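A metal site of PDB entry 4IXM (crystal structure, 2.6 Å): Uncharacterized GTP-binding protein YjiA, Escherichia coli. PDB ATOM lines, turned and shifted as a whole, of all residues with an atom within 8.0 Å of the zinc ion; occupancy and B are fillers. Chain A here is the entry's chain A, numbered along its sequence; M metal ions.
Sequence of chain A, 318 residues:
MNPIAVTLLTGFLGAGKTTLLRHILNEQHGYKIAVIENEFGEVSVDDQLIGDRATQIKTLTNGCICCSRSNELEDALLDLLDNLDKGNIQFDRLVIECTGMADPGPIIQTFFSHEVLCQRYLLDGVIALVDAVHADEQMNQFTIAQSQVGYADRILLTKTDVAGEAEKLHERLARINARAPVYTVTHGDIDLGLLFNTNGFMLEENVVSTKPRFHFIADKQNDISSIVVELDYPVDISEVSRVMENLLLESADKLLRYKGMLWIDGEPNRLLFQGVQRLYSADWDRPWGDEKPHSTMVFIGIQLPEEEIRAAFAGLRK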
ATOM      1  N   LEU A  21      13.835  27.108  26.708  1.00  0.00           N
ATOM      2  CA  LEU A  21      13.564  25.866  26.005  1.00  0.00           C
ATOM      3  C   LEU A  21      12.545  26.072  24.890  1.00  0.00           C
ATOM      4  O   LEU A  21      12.640  25.472  23.825  1.00  0.00           O
ATOM      5  CB  LEU A  21      13.056  24.801  26.977  1.00  0.00           C
ATOM      6  CG  LEU A  21      14.073  23.793  27.517  1.00  0.00           C
ATOM      7  CD1 LEU A  21      15.326  24.482  28.009  1.00  0.00           C
ATOM      8  CD2 LEU A  21      13.451  22.943  28.616  1.00  0.00           C
ATOM      9  N   LEU A  25      13.189  25.247  20.731  1.00  0.00           N
ATOM     10  CA  LEU A  25      12.379  24.251  20.035  1.00  0.00           C
ATOM     11  C   LEU A  25      11.479  24.848  18.961  1.00  0.00           C
ATOM     12  O   LEU A  25      11.140  24.187  17.981  1.00  0.00           O
ATOM     13  CB  LEU A  25      11.544  23.457  21.043  1.00  0.00           C
ATOM     14  CG  LEU A  25      12.335  22.729  22.134  1.00  0.00           C
ATOM     15  CD1 LEU A  25      11.413  22.252  23.241  1.00  0.00           C
ATOM     16  CD2 LEU A  25      13.120  21.576  21.533  1.00  0.00           C
ATOM     17  N   VAL A  35      17.413  18.395  21.545  1.00  0.00           N
ATOM     18  CA  VAL A  35      17.126  18.707  22.939  1.00  0.00           C
ATOM     19  C   VAL A  35      16.558  17.511  23.705  1.00  0.00           C
ATOM     20  O   VAL A  35      15.593  16.885  23.261  1.00  0.00           O
ATOM     21  CB  VAL A  35      16.132  19.896  23.063  1.00  0.00           C
ATOM     22  CG1 VAL A  35      15.753  20.124  24.519  1.00  0.00           C
ATOM     23  CG2 VAL A  35      16.733  21.155  22.460  1.00  0.00           C
ATOM     24  N   ILE A  36      17.163  17.213  24.842  1.00  0.00           N
ATOM     25  CA  ILE A  36      16.602  16.240  25.782  1.00  0.00           C
ATOM     26  C   ILE A  36      16.062  16.981  26.994  1.00  0.00           C
ATOM     27  O   ILE A  36      16.824  17.545  27.793  1.00  0.00           O
ATOM     28  CB  ILE A  36      17.649  15.211  26.226  1.00  0.00           C
ATOM     29  CG1 ILE A  36      18.113  14.368  25.028  1.00  0.00           C
ATOM     30  CG2 ILE A  36      17.092  14.314  27.320  1.00  0.00           C
ATOM     31  CD1 ILE A  36      19.035  13.232  25.404  1.00  0.00           C
ATOM     32  N   GLU A  37      14.741  16.990  27.136  1.00  0.00           N
ATOM     33  CA  GLU A  37      14.101  17.751  28.200  1.00  0.00           C
ATOM     34  C   GLU A  37      13.105  16.902  28.984  1.00  0.00           C
ATOM     35  O   GLU A  37      12.820  15.766  28.626  1.00  0.00           O
ATOM     36  CB  GLU A  37      13.396  18.983  27.623  1.00  0.00           C
ATOM     37  CG  GLU A  37      12.323  18.643  26.602  1.00  0.00           C
ATOM     38  CD  GLU A  37      11.373  19.806  26.345  1.00  0.00           C
ATOM     39  OE1 GLU A  37      10.654  19.774  25.321  1.00  0.00           O
ATOM     40  OE2 GLU A  37      11.338  20.748  27.170  1.00  0.00           O
ATOM     41  N   ASN A  38      12.579  17.481  30.056  1.00  0.00           N
ATOM     42  CA  ASN A  38      11.630  16.792  30.918  1.00  0.00           C
ATOM     43  C   ASN A  38      10.192  17.063  30.516  1.00  0.00           C
ATOM     44  O   ASN A  38       9.321  16.199  30.656  1.00  0.00           O
ATOM     45  CB  ASN A  38      11.853  17.172  32.384  1.00  0.00           C
ATOM     46  CG  ASN A  38      13.273  16.904  32.847  1.00  0.00           C
ATOM     47  OD1 ASN A  38      13.929  15.966  32.384  1.00  0.00           O
ATOM     48  ND2 ASN A  38      13.751  17.727  33.777  1.00  0.00           N
ATOM     49  N   GLU A  39       9.936  18.269  30.008  1.00  0.00           N
ATOM     50  CA  GLU A  39       8.581  18.681  29.671  1.00  0.00           C
ATOM     51  C   GLU A  39       8.279  18.512  28.180  1.00  0.00           C
ATOM     52  O   GLU A  39       8.669  17.512  27.564  1.00  0.00           O
ATOM     53  CB  GLU A  39       8.313  20.128  30.111  1.00  0.00           C
ATOM     54  N   PHE A  40       7.575  19.482  27.608  1.00  0.00           N
ATOM     55  CA  PHE A  40       7.062  19.377  26.256  1.00  0.00           C
ATOM     56  C   PHE A  40       6.798  20.801  25.769  1.00  0.00           C
ATOM     57  O   PHE A  40       5.673  21.295  25.835  1.00  0.00           O
ATOM     58  CB  PHE A  40       5.763  18.544  26.259  1.00  0.00           C
ATOM     59  CG  PHE A  40       5.136  18.372  24.905  1.00  0.00           C
ATOM     60  CD1 PHE A  40       5.557  17.365  24.053  1.00  0.00           C
ATOM     61  CD2 PHE A  40       4.081  19.179  24.495  1.00  0.00           C
ATOM     62  CE1 PHE A  40       4.978  17.187  22.817  1.00  0.00           C
ATOM     63  CE2 PHE A  40       3.494  19.009  23.250  1.00  0.00           C
ATOM     64  CZ  PHE A  40       3.942  18.009  22.414  1.00  0.00           C
ATOM     65  N   GLY A  41       7.853  21.470  25.309  1.00  0.00           N
ATOM     66  CA  GLY A  41       7.767  22.858  24.926  1.00  0.00           C
ATOM     67  C   GLY A  41       7.473  23.070  23.463  1.00  0.00           C
ATOM     68  O   GLY A  41       6.792  24.029  23.090  1.00  0.00           O
ATOM     69  N   GLU A  42       7.985  22.179  22.618  1.00  0.00           N
ATOM     70  CA  GLU A  42       7.757  22.265  21.182  1.00  0.00           C
ATOM     71  C   GLU A  42       6.273  22.134  20.842  1.00  0.00           C
ATOM     72  O   GLU A  42       5.518  21.481  21.551  1.00  0.00           O
ATOM     73  CB  GLU A  42       8.566  21.207  20.432  1.00  0.00           C
ATOM     74  CG  GLU A  42       9.143  20.109  21.320  1.00  0.00           C
ATOM     75  CD  GLU A  42       8.093  19.173  21.874  1.00  0.00           C
ATOM     76  OE1 GLU A  42       7.019  19.050  21.253  1.00  0.00           O
ATOM     77  OE2 GLU A  42       8.337  18.571  22.938  1.00  0.00           O
ATOM     78  N   VAL A  43       5.871  22.776  19.747  1.00  0.00           N
ATOM     79  CA  VAL A  43       4.476  22.745  19.316  1.00  0.00           C
ATOM     80  C   VAL A  43       4.348  22.151  17.923  1.00  0.00           C
ATOM     81  O   VAL A  43       3.473  21.318  17.670  1.00  0.00           O
ATOM     82  CB  VAL A  43       3.850  24.157  19.324  1.00  0.00           C
ATOM     83  N   VAL A  45       5.610  19.733  15.721  1.00  0.00           N
ATOM     84  CA  VAL A  45       6.363  18.508  15.498  1.00  0.00           C
ATOM     85  C   VAL A  45       6.221  18.066  14.044  1.00  0.00           C
ATOM     86  O   VAL A  45       5.128  17.719  13.595  1.00  0.00           O
ATOM     87  CB  VAL A  45       5.894  17.376  16.417  1.00  0.00           C
ATOM     88  CG1 VAL A  45       6.723  16.125  16.186  1.00  0.00           C
ATOM     89  CG2 VAL A  45       5.981  17.816  17.883  1.00  0.00           C
ATOM     90  N   LYS A  58      11.761  13.240  17.909  1.00  0.00           N
ATOM     91  CA  LYS A  58      10.899  14.138  17.142  1.00  0.00           C
ATOM     92  C   LYS A  58      11.675  15.213  16.387  1.00  0.00           C
ATOM     93  O   LYS A  58      12.479  15.932  16.973  1.00  0.00           O
ATOM     94  CB  LYS A  58       9.875  14.818  18.060  1.00  0.00           C
ATOM     95  CG  LYS A  58       8.895  13.870  18.731  1.00  0.00           C
ATOM     96  CD  LYS A  58       7.893  14.640  19.573  1.00  0.00           C
ATOM     97  CE  LYS A  58       6.910  13.699  20.251  1.00  0.00           C
ATOM     98  NZ  LYS A  58       5.900  14.450  21.052  1.00  0.00           N
ATOM     99  N   LEU A  60      11.643  18.743  14.455  1.00  0.00           N
ATOM    100  CA  LEU A  60      10.823  19.947  14.523  1.00  0.00           C
ATOM    101  C   LEU A  60      10.866  20.769  13.235  1.00  0.00           C
ATOM    102  O   LEU A  60      11.710  20.541  12.375  1.00  0.00           O
ATOM    103  CB  LEU A  60      11.252  20.803  15.714  1.00  0.00           C
ATOM    104  CG  LEU A  60      11.326  20.081  17.059  1.00  0.00           C
ATOM    105  CD1 LEU A  60      11.785  21.029  18.148  1.00  0.00           C
ATOM    106  CD2 LEU A  60       9.989  19.459  17.413  1.00  0.00           C
ATOM    107  N   ILE A  65      15.702  19.107  16.923  1.00  0.00           N
ATOM    108  CA  ILE A  65      15.208  17.781  17.288  1.00  0.00           C
ATOM    109  C   ILE A  65      14.835  17.760  18.766  1.00  0.00           C
ATOM    110  O   ILE A  65      15.575  18.271  19.607  1.00  0.00           O
ATOM    111  CB  ILE A  65      16.283  16.702  17.033  1.00  0.00           C
ATOM    112  CG1 ILE A  65      16.817  16.803  15.603  1.00  0.00           C
ATOM    113  CG2 ILE A  65      15.739  15.322  17.319  1.00  0.00           C
ATOM    114  CD1 ILE A  65      15.799  16.453  14.539  1.00  0.00           C
ATOM    115  N   CYS A  66      13.697  17.154  19.085  1.00  0.00           N
ATOM    116  CA  CYS A  66      13.313  16.939  20.473  1.00  0.00           C
ATOM    117  C   CYS A  66      13.367  15.455  20.795  1.00  0.00           C
ATOM    118  O   CYS A  66      12.804  14.630  20.075  1.00  0.00           O
ATOM    119  CB  CYS A  66      11.930  17.511  20.761  1.00  0.00           C
ATOM    120  SG  CYS A  66      11.583  17.722  22.522  1.00  0.00           S
ATOM    121  N   CYS A  67      14.034  15.118  21.904  1.00  0.00           N
ATOM    122  CA  CYS A  67      14.293  13.725  22.236  1.00  0.00           C
ATOM    123  C   CYS A  67      13.912  13.414  23.684  1.00  0.00           C
ATOM    124  O   CYS A  67      14.060  14.252  24.566  1.00  0.00           O
ATOM    125  CB  CYS A  67      15.771  13.400  22.002  1.00  0.00           C
ATOM    126  SG  CYS A  67      16.219  11.687  22.311  1.00  0.00           S
ATOM    127  N   SER A  68      13.420  12.203  23.902  1.00  0.00           N
ATOM    128  CA  SER A  68      13.065  11.752  25.237  1.00  0.00           C
ATOM    129  C   SER A  68      14.186  10.879  25.811  1.00  0.00           C
ATOM    130  O   SER A  68      15.056  10.418  25.076  1.00  0.00           O
ATOM    131  CB  SER A  68      11.754  10.963  25.209  1.00  0.00           C
ATOM    132  OG  SER A  68      11.899   9.779  24.446  1.00  0.00           O
ATOM    133  N   GLU A  97      18.660  18.907  29.527  1.00  0.00           N
ATOM    134  CA  GLU A  97      18.123  19.572  30.698  1.00  0.00           C
ATOM    135  C   GLU A  97      18.363  18.747  31.953  1.00  0.00           C
ATOM    136  O   GLU A  97      17.962  17.589  32.039  1.00  0.00           O
ATOM    137  CB  GLU A  97      16.621  19.835  30.535  1.00  0.00           C
ATOM    138  CG  GLU A  97      15.980  20.502  31.740  1.00  0.00           C
ATOM    139  CD  GLU A  97      14.469  20.533  31.648  1.00  0.00           C
ATOM    140  OE1 GLU A  97      13.937  20.364  30.531  1.00  0.00           O
ATOM    141  OE2 GLU A  97      13.809  20.713  32.696  1.00  0.00           O
HETATM  142 ZN    ZN M   1       9.999  18.100  24.181  1.00  0.00          ZN
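Glu 39 touches the zinc ion. Phe 40 touches the zinc ion (CA to ZN, 3.8 Å). Of the 19 residues printed, 5 come within 4 Å of the zinc ion.
The zinc ion is bound by OE1 of Glu 37 (2.1 Å), OE2 of Glu 42 (2.1 Å) and SG of Cys 66 (2.3 Å). The zinc ion has three donor atoms within binding distance.
The backbone NH (N) of Gly 41 lies close to the side-chain carboxylate (OE1) of Glu 37 (3.3 Å). O of Lys 58 sits at hydrogen-bond distance from N of Cys 66, at 2.7 Å.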
